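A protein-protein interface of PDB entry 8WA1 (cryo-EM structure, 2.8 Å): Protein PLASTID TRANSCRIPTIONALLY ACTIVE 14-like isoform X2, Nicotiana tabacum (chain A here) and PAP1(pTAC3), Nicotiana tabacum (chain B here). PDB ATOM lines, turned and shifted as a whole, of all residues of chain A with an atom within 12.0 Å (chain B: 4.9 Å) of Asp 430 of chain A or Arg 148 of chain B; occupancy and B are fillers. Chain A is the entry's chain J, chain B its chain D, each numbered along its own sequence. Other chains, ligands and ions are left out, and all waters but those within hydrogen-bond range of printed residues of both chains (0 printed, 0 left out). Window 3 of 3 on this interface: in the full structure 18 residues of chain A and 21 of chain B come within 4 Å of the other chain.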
ATOM      1  N   HIS A 381      31.873 -19.250  37.286  1.00  0.00           N
ATOM      2  CA  HIS A 381      31.679 -18.349  36.158  1.00  0.00           C
ATOM      3  C   HIS A 381      32.594 -18.754  35.010  1.00  0.00           C
ATOM      4  O   HIS A 381      33.818 -18.800  35.165  1.00  0.00           O
ATOM      5  CB  HIS A 381      31.944 -16.900  36.561  1.00  0.00           C
ATOM      6  CG  HIS A 381      31.400 -15.898  35.592  1.00  0.00           C
ATOM      7  ND1 HIS A 381      30.080 -15.501  35.597  1.00  0.00           N
ATOM      8  CD2 HIS A 381      31.993 -15.220  34.582  1.00  0.00           C
ATOM      9  CE1 HIS A 381      29.885 -14.617  34.634  1.00  0.00           C
ATOM     10  NE2 HIS A 381      31.030 -14.429  34.003  1.00  0.00           N
ATOM     11  N   LEU A 382      31.995 -19.037  33.853  1.00  0.00           N
ATOM     12  CA  LEU A 382      32.760 -19.554  32.722  1.00  0.00           C
ATOM     13  C   LEU A 382      33.668 -18.484  32.128  1.00  0.00           C
ATOM     14  O   LEU A 382      34.834 -18.751  31.807  1.00  0.00           O
ATOM     15  CB  LEU A 382      31.806 -20.106  31.661  1.00  0.00           C
ATOM     16  CG  LEU A 382      32.434 -20.671  30.387  1.00  0.00           C
ATOM     17  CD1 LEU A 382      33.382 -21.813  30.712  1.00  0.00           C
ATOM     18  CD2 LEU A 382      31.352 -21.127  29.421  1.00  0.00           C
ATOM     19  N   ASP A 383      33.149 -17.264  31.963  1.00  0.00           N
ATOM     20  CA  ASP A 383      33.932 -16.212  31.324  1.00  0.00           C
ATOM     21  C   ASP A 383      35.158 -15.841  32.145  1.00  0.00           C
ATOM     22  O   ASP A 383      36.262 -15.749  31.597  1.00  0.00           O
ATOM     23  CB  ASP A 383      33.065 -14.977  31.085  1.00  0.00           C
ATOM     24  CG  ASP A 383      33.772 -13.914  30.260  1.00  0.00           C
ATOM     25  OD1 ASP A 383      34.717 -13.275  30.772  1.00  0.00           O
ATOM     26  OD2 ASP A 383      33.390 -13.728  29.087  1.00  0.00           O
ATOM     27  N   THR A 384      34.988 -15.638  33.452  1.00  0.00           N
ATOM     28  CA  THR A 384      36.126 -15.287  34.294  1.00  0.00           C
ATOM     29  C   THR A 384      37.129 -16.430  34.363  1.00  0.00           C
ATOM     30  O   THR A 384      38.341 -16.196  34.430  1.00  0.00           O
ATOM     31  CB  THR A 384      35.640 -14.905  35.693  1.00  0.00           C
ATOM     32  OG1 THR A 384      34.643 -13.881  35.587  1.00  0.00           O
ATOM     33  CG2 THR A 384      36.793 -14.390  36.539  1.00  0.00           C
ATOM     34  N   SER A 387      39.065 -16.378  31.232  1.00  0.00           N
ATOM     35  CA  SER A 387      39.927 -15.201  31.249  1.00  0.00           C
ATOM     36  C   SER A 387      41.168 -15.435  32.099  1.00  0.00           C
ATOM     37  O   SER A 387      42.290 -15.162  31.655  1.00  0.00           O
ATOM     38  CB  SER A 387      39.152 -13.986  31.761  1.00  0.00           C
ATOM     39  OG  SER A 387      38.038 -13.702  30.932  1.00  0.00           O
ATOM     40  N   LEU A 394      35.260 -20.344  20.733  1.00  0.00           N
ATOM     41  CA  LEU A 394      33.906 -20.792  21.005  1.00  0.00           C
ATOM     42  C   LEU A 394      33.938 -22.071  21.831  1.00  0.00           C
ATOM     43  O   LEU A 394      34.962 -22.754  21.903  1.00  0.00           O
ATOM     44  CB  LEU A 394      33.162 -20.991  19.687  1.00  0.00           C
ATOM     45  CG  LEU A 394      33.031 -19.740  18.814  1.00  0.00           C
ATOM     46  CD1 LEU A 394      32.320 -20.063  17.512  1.00  0.00           C
ATOM     47  CD2 LEU A 394      32.306 -18.635  19.564  1.00  0.00           C
ATOM     48  N   PRO A 395      32.824 -22.424  22.480  1.00  0.00           N
ATOM     49  CA  PRO A 395      32.800 -23.674  23.258  1.00  0.00           C
ATOM     50  C   PRO A 395      33.135 -24.908  22.439  1.00  0.00           C
ATOM     51  O   PRO A 395      33.551 -25.923  23.010  1.00  0.00           O
ATOM     52  CB  PRO A 395      31.361 -23.722  23.789  1.00  0.00           C
ATOM     53  CG  PRO A 395      30.945 -22.295  23.857  1.00  0.00           C
ATOM     54  CD  PRO A 395      31.600 -21.627  22.683  1.00  0.00           C
ATOM     55  N   TRP A 426      27.795 -20.904  34.844  1.00  0.00           N
ATOM     56  CA  TRP A 426      26.647 -20.019  34.706  1.00  0.00           C
ATOM     57  C   TRP A 426      27.074 -18.756  33.971  1.00  0.00           C
ATOM     58  O   TRP A 426      28.124 -18.180  34.274  1.00  0.00           O
ATOM     59  CB  TRP A 426      26.051 -19.665  36.075  1.00  0.00           C
ATOM     60  CG  TRP A 426      26.945 -18.812  36.927  1.00  0.00           C
ATOM     61  CD1 TRP A 426      27.918 -19.241  37.782  1.00  0.00           C
ATOM     62  CD2 TRP A 426      26.943 -17.382  37.004  1.00  0.00           C
ATOM     63  NE1 TRP A 426      28.525 -18.165  38.385  1.00  0.00           N
ATOM     64  CE2 TRP A 426      27.945 -17.013  37.925  1.00  0.00           C
ATOM     65  CE3 TRP A 426      26.195 -16.378  36.384  1.00  0.00           C
ATOM     66  CZ2 TRP A 426      28.214 -15.683  38.241  1.00  0.00           C
ATOM     67  CZ3 TRP A 426      26.465 -15.058  36.698  1.00  0.00           C
ATOM     68  CH2 TRP A 426      27.465 -14.723  37.618  1.00  0.00           C
ATOM     69  N   SER A 427      26.268 -18.338  32.998  1.00  0.00           N
ATOM     70  CA  SER A 427      26.517 -17.118  32.238  1.00  0.00           C
ATOM     71  C   SER A 427      25.206 -16.365  32.090  1.00  0.00           C
ATOM     72  O   SER A 427      24.278 -16.855  31.438  1.00  0.00           O
ATOM     73  CB  SER A 427      27.116 -17.432  30.863  1.00  0.00           C
ATOM     74  OG  SER A 427      27.384 -16.241  30.143  1.00  0.00           O
ATOM     75  N   ASP A 428      25.127 -15.181  32.691  1.00  0.00           N
ATOM     76  CA  ASP A 428      23.917 -14.367  32.659  1.00  0.00           C
ATOM     77  C   ASP A 428      24.269 -12.981  32.144  1.00  0.00           C
ATOM     78  O   ASP A 428      24.534 -12.072  32.938  1.00  0.00           O
ATOM     79  CB  ASP A 428      23.273 -14.278  34.046  1.00  0.00           C
ATOM     80  CG  ASP A 428      21.870 -13.706  34.005  1.00  0.00           C
ATOM     81  OD1 ASP A 428      21.334 -13.518  32.894  1.00  0.00           O
ATOM     82  OD2 ASP A 428      21.306 -13.446  35.087  1.00  0.00           O
ATOM     83  N   GLY A 429      24.247 -12.818  30.824  1.00  0.00           N
ATOM     84  CA  GLY A 429      24.539 -11.526  30.227  1.00  0.00           C
ATOM     85  C   GLY A 429      25.909 -11.013  30.621  1.00  0.00           C
ATOM     86  O   GLY A 429      26.918 -11.722  30.520  1.00  0.00           O
ATOM     87  N   ASP A 430      25.951  -9.765  31.089  1.00  0.00           N
ATOM     88  CA  ASP A 430      27.190  -9.125  31.511  1.00  0.00           C
ATOM     89  C   ASP A 430      27.238  -8.879  33.013  1.00  0.00           C
ATOM     90  O   ASP A 430      27.970  -7.989  33.461  1.00  0.00           O
ATOM     91  CB  ASP A 430      27.395  -7.807  30.757  1.00  0.00           C
ATOM     92  CG  ASP A 430      27.642  -8.017  29.278  1.00  0.00           C
ATOM     93  OD1 ASP A 430      27.754  -9.187  28.853  1.00  0.00           O
ATOM     94  OD2 ASP A 430      27.725  -7.014  28.538  1.00  0.00           O
ATOM     95  N   LEU A 431      26.475  -9.634  33.797  1.00  0.00           N
ATOM     96  CA  LEU A 431      26.522  -9.482  35.243  1.00  0.00           C
ATOM     97  C   LEU A 431      27.903  -9.879  35.760  1.00  0.00           C
ATOM     98  O   LEU A 431      28.411 -10.953  35.413  1.00  0.00           O
ATOM     99  CB  LEU A 431      25.443 -10.339  35.905  1.00  0.00           C
ATOM    100  CG  LEU A 431      25.305 -10.255  37.427  1.00  0.00           C
ATOM    101  CD1 LEU A 431      24.822  -8.877  37.848  1.00  0.00           C
ATOM    102  CD2 LEU A 431      24.364 -11.334  37.942  1.00  0.00           C
ATOM    103  N   PRO A 432      28.537  -9.048  36.580  1.00  0.00           N
ATOM    104  CA  PRO A 432      29.870  -9.379  37.090  1.00  0.00           C
ATOM    105  C   PRO A 432      29.788 -10.410  38.201  1.00  0.00           C
ATOM    106  O   PRO A 432      28.823 -10.423  38.980  1.00  0.00           O
ATOM    107  CB  PRO A 432      30.389  -8.033  37.614  1.00  0.00           C
ATOM    108  CG  PRO A 432      29.154  -7.286  37.981  1.00  0.00           C
ATOM    109  CD  PRO A 432      28.111  -7.695  36.977  1.00  0.00           C
ATOM    110  N   PRO A 433      30.781 -11.291  38.305  1.00  0.00           N
ATOM    111  CA  PRO A 433      30.745 -12.319  39.351  1.00  0.00           C
ATOM    112  C   PRO A 433      30.962 -11.720  40.733  1.00  0.00           C
ATOM    113  O   PRO A 433      31.621 -10.689  40.891  1.00  0.00           O
ATOM    114  CB  PRO A 433      31.891 -13.262  38.963  1.00  0.00           C
ATOM    115  CG  PRO A 433      32.188 -12.951  37.525  1.00  0.00           C
ATOM    116  CD  PRO A 433      31.899 -11.494  37.372  1.00  0.00           C
ATOM    117  N   ILE A 434      30.401 -12.379  41.736  1.00  0.00           N
ATOM    118  CA  ILE A 434      30.548 -11.985  43.134  1.00  0.00           C
ATOM    119  C   ILE A 434      31.652 -12.834  43.755  1.00  0.00           C
ATOM    120  O   ILE A 434      31.634 -14.061  43.589  1.00  0.00           O
ATOM    121  CB  ILE A 434      29.227 -12.153  43.909  1.00  0.00           C
ATOM    122  CG1 ILE A 434      28.167 -11.198  43.358  1.00  0.00           C
ATOM    123  CG2 ILE A 434      29.439 -11.917  45.396  1.00  0.00           C
ATOM    124  CD1 ILE A 434      28.570  -9.742  43.428  1.00  0.00           C
ATOM    125  N   VAL B 113      31.363  -2.513  33.499  1.00  0.00           N
ATOM    126  CA  VAL B 113      30.053  -3.160  33.455  1.00  0.00           C
ATOM    127  C   VAL B 113      29.003  -2.304  34.152  1.00  0.00           C
ATOM    128  O   VAL B 113      27.823  -2.340  33.783  1.00  0.00           O
ATOM    129  CB  VAL B 113      30.111  -4.581  34.050  1.00  0.00           C
ATOM    130  CG1 VAL B 113      31.079  -5.450  33.257  1.00  0.00           C
ATOM    131  CG2 VAL B 113      30.485  -4.547  35.521  1.00  0.00           C
ATOM    132  N   VAL B 116      27.993  -0.007  31.547  1.00  0.00           N
ATOM    133  CA  VAL B 116      27.260  -0.691  30.483  1.00  0.00           C
ATOM    134  C   VAL B 116      25.821  -0.956  30.906  1.00  0.00           C
ATOM    135  O   VAL B 116      24.880  -0.736  30.133  1.00  0.00           O
ATOM    136  CB  VAL B 116      27.981  -1.995  30.088  1.00  0.00           C
ATOM    137  CG1 VAL B 116      27.085  -2.852  29.212  1.00  0.00           C
ATOM    138  CG2 VAL B 116      29.284  -1.689  29.367  1.00  0.00           C
ATOM    139  N   GLU B 141      36.479  -9.666  28.705  1.00  0.00           N
ATOM    140  CA  GLU B 141      35.091  -9.408  29.074  1.00  0.00           C
ATOM    141  C   GLU B 141      34.746  -7.930  28.938  1.00  0.00           C
ATOM    142  O   GLU B 141      33.634  -7.579  28.528  1.00  0.00           O
ATOM    143  CB  GLU B 141      34.831  -9.894  30.500  1.00  0.00           C
ATOM    144  CG  GLU B 141      33.479  -9.485  31.070  1.00  0.00           C
ATOM    145  CD  GLU B 141      32.309 -10.079  30.315  1.00  0.00           C
ATOM    146  OE1 GLU B 141      32.463 -11.176  29.739  1.00  0.00           O
ATOM    147  OE2 GLU B 141      31.232  -9.447  30.298  1.00  0.00           O
ATOM    148  N   LEU B 144      34.291  -7.263  25.314  1.00  0.00           N
ATOM    149  CA  LEU B 144      33.045  -7.893  24.888  1.00  0.00           C
ATOM    150  C   LEU B 144      31.839  -7.055  25.292  1.00  0.00           C
ATOM    151  O   LEU B 144      30.902  -6.880  24.506  1.00  0.00           O
ATOM    152  CB  LEU B 144      32.938  -9.299  25.479  1.00  0.00           C
ATOM    153  CG  LEU B 144      31.703 -10.108  25.074  1.00  0.00           C
ATOM    154  CD1 LEU B 144      31.986 -10.939  23.831  1.00  0.00           C
ATOM    155  CD2 LEU B 144      31.220 -10.984  26.222  1.00  0.00           C
ATOM    156  N   ALA B 145      31.849  -6.523  26.517  1.00  0.00           N
ATOM    157  CA  ALA B 145      30.743  -5.686  26.970  1.00  0.00           C
ATOM    158  C   ALA B 145      30.676  -4.390  26.175  1.00  0.00           C
ATOM    159  O   ALA B 145      29.584  -3.912  25.840  1.00  0.00           O
ATOM    160  CB  ALA B 145      30.881  -5.397  28.464  1.00  0.00           C
ATOM    161  N   LEU B 146      31.834  -3.806  25.858  1.00  0.00           N
ATOM    162  CA  LEU B 146      31.847  -2.597  25.040  1.00  0.00           C
ATOM    163  C   LEU B 146      31.305  -2.869  23.641  1.00  0.00           C
ATOM    164  O   LEU B 146      30.538  -2.064  23.098  1.00  0.00           O
ATOM    165  CB  LEU B 146      33.262  -2.027  24.969  1.00  0.00           C
ATOM    166  CG  LEU B 146      33.856  -1.546  26.293  1.00  0.00           C
ATOM    167  CD1 LEU B 146      35.286  -1.073  26.099  1.00  0.00           C
ATOM    168  CD2 LEU B 146      33.002  -0.444  26.894  1.00  0.00           C
ATOM    169  N   VAL B 147      31.689  -4.001  23.046  1.00  0.00           N
ATOM    170  CA  VAL B 147      31.184  -4.370  21.727  1.00  0.00           C
ATOM    171  C   VAL B 147      29.677  -4.591  21.776  1.00  0.00           C
ATOM    172  O   VAL B 147      28.944  -4.175  20.873  1.00  0.00           O
ATOM    173  CB  VAL B 147      31.926  -5.615  21.205  1.00  0.00           C
ATOM    174  CG1 VAL B 147      31.148  -6.272  20.081  1.00  0.00           C
ATOM    175  CG2 VAL B 147      33.321  -5.241  20.734  1.00  0.00           C
ATOM    176  N   ARG B 148      29.192  -5.243  22.835  1.00  0.00           N
ATOM    177  CA  ARG B 148      27.757  -5.470  22.969  1.00  0.00           C
ATOM    178  C   ARG B 148      27.000  -4.154  23.114  1.00  0.00           C
ATOM    179  O   ARG B 148      25.928  -3.979  22.521  1.00  0.00           O
ATOM    180  CB  ARG B 148      27.485  -6.385  24.163  1.00  0.00           C
ATOM    181  CG  ARG B 148      26.015  -6.642  24.436  1.00  0.00           C
ATOM    182  CD  ARG B 148      25.823  -7.599  25.604  1.00  0.00           C
ATOM    183  NE  ARG B 148      26.199  -8.971  25.271  1.00  0.00           N
ATOM    184  CZ  ARG B 148      27.366  -9.528  25.579  1.00  0.00           C
ATOM    185  NH1 ARG B 148      28.285  -8.834  26.236  1.00  0.00           N
ATOM    186  NH2 ARG B 148      27.614 -10.784  25.232  1.00  0.00           N
ATOM    187  N   LEU B 149      27.545  -3.216  23.893  1.00  0.00           N
ATOM    188  CA  LEU B 149      26.897  -1.918  24.049  1.00  0.00           C
ATOM    189  C   LEU B 149      26.886  -1.149  22.735  1.00  0.00           C
ATOM    190  O   LEU B 149      25.884  -0.508  22.391  1.00  0.00           O
ATOM    191  CB  LEU B 149      27.599  -1.108  25.139  1.00  0.00           C
ATOM    192  CG  LEU B 149      26.723  -0.353  26.145  1.00  0.00           C
ATOM    193  CD1 LEU B 149      27.582   0.530  27.034  1.00  0.00           C
ATOM    194  CD2 LEU B 149      25.643   0.471  25.457  1.00  0.00           C
ATOM    195  N   PHE B 150      27.989  -1.199  21.983  1.00  0.00           N
ATOM    196  CA  PHE B 150      28.031  -0.510  20.695  1.00  0.00           C
ATOM    197  C   PHE B 150      27.069  -1.142  19.698  1.00  0.00           C
ATOM    198  O   PHE B 150      26.465  -0.440  18.878  1.00  0.00           O
ATOM    199  CB  PHE B 150      29.457  -0.514  20.141  1.00  0.00           C
ATOM    200  CG  PHE B 150      30.375   0.456  20.826  1.00  0.00           C
ATOM    201  CD1 PHE B 150      29.867   1.544  21.514  1.00  0.00           C
ATOM    202  CD2 PHE B 150      31.746   0.281  20.777  1.00  0.00           C
ATOM    203  CE1 PHE B 150      30.710   2.439  22.143  1.00  0.00           C
ATOM    204  CE2 PHE B 150      32.594   1.171  21.405  1.00  0.00           C
ATOM    205  CZ  PHE B 150      32.076   2.251  22.089  1.00  0.00           C
ATOM    206  N   GLY B 151      26.915  -2.466  19.749  1.00  0.00           N
ATOM    207  CA  GLY B 151      25.965  -3.121  18.867  1.00  0.00           C
ATOM    208  C   GLY B 151      24.528  -2.804  19.228  1.00  0.00           C
ATOM    209  O   GLY B 151      23.671  -2.676  18.350  1.00  0.00           O
ATOM    210  N   ALA B 152      24.244  -2.671  20.526  1.00  0.00           N
ATOM    211  CA  ALA B 152      22.896  -2.316  20.957  1.00  0.00           C
ATOM    212  C   ALA B 152      22.524  -0.908  20.507  1.00  0.00           C
ATOM    213  O   ALA B 152      21.393  -0.665  20.069  1.00  0.00           O
ATOM    214  CB  ALA B 152      22.781  -2.444  22.475  1.00  0.00           C
ATOM    215  N   VAL B 179      29.331 -11.479  18.236  1.00  0.00           N
ATOM    216  CA  VAL B 179      28.418 -10.767  19.128  1.00  0.00           C
ATOM    217  C   VAL B 179      28.044  -9.416  18.532  1.00  0.00           C
ATOM    218  O   VAL B 179      26.889  -8.980  18.619  1.00  0.00           O
ATOM    219  CB  VAL B 179      29.045 -10.621  20.527  1.00  0.00           C
ATOM    220  CG1 VAL B 179      28.223  -9.676  21.387  1.00  0.00           C
ATOM    221  CG2 VAL B 179      29.161 -11.981  21.195  1.00  0.00           C
ATOM    222  N   GLU B 183      24.231  -8.386  17.613  1.00  0.00           N
ATOM    223  CA  GLU B 183      23.577  -7.235  18.228  1.00  0.00           C
ATOM    224  C   GLU B 183      23.147  -6.217  17.181  1.00  0.00           C
ATOM    225  O   GLU B 183      22.098  -5.579  17.326  1.00  0.00           O
ATOM    226  CB  GLU B 183      24.503  -6.591  19.259  1.00  0.00           C
ATOM    227  CG  GLU B 183      24.746  -7.441  20.496  1.00  0.00           C
ATOM    228  CD  GLU B 183      23.511  -7.581  21.367  1.00  0.00           C
ATOM    229  OE1 GLU B 183      22.606  -6.725  21.266  1.00  0.00           O
ATOM    230  OE2 GLU B 183      23.445  -8.548  22.155  1.00  0.00           O
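The side-chain carboxylate of Asp 430 of chain A is in salt-bridge range of the guanidinium group of Arg 148 of chain B (2.7 Å). The side-chain carboxylate (OE1) of Glu 141 of chain B sits close to the side-chain carboxylate (OD2) of Asp 383 of chain A.
O of Asp 383 of chain A is in hydrogen-bond range of OG of Ser 387 of chain A (2.8 Å).
Asp 430 of chain A touches Glu 141 of chain B (OD1 to OE2, 3.8 Å). OD2 of Asp 430 of chain A touches CB of Ala 145 of chain B, 3.5 Å away. Val 113 of chain B touches Pro 432 of chain A (CG2 to CG, 3.9 Å).
Of the printed residues of chain B, Asp 430 of chain A touches Glu 141, Ala 145 and Arg 148. No residue of chain A comes within 4 Å of Val 116 of chain B. No residue of chain A comes within 4 Å of Leu 144 of chain B. Of the printed residues of chain A, Ala 145 of chain B touches Asp 430 (3.5 Å). No residue of chain A comes within 4 Å of Val 147 of chain B. No residue of chain A comes within 4 Å of Gly 151 of chain B. No residue of chain A comes within 4 Å of Ala 152 of chain B. No residue of chain A comes within 4 Å of Val 179 of chain B. No residue of chain A comes within 4 Å of Glu 183 of chain B. Of the printed residues of chain A, Val 113 of chain B touches Pro 432. Of the printed residues of chain B, Pro 432 of chain A touches Val 113. Of the printed residues of chain B, Asp 383 of chain A touches Glu 141. Printed residues of chain A within 4 Å of Glu 141 of chain B: Asp 383 and Asp 430. Pro 433 of chain A touches none of the printed residues of chain B. The nearest printed residue of chain B that does not touch Asp 430 of chain A is Val 113 of chain B (4.02 Å).
Of the 14 printed residues of chain B, 4 touch a printed residue of chain A. Printed residues of chain B that touch a printed residue of chain A: Val 113, Glu 141, Ala 145 and Arg 148. Hydrophobic or aromatic side chains of chain B within 4 Å of the printed part of chain A: Val 113 and Ala 145. Of the 16 printed residues of chain A, 3 touch a printed residue of chain B. Among the printed residues, Asp or Glu carboxylates within 4 Å of a Lys or Arg side-chain nitrogen of the other chain: Asp 430 of chain A with Arg 148 of chain B (2.7 Å).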
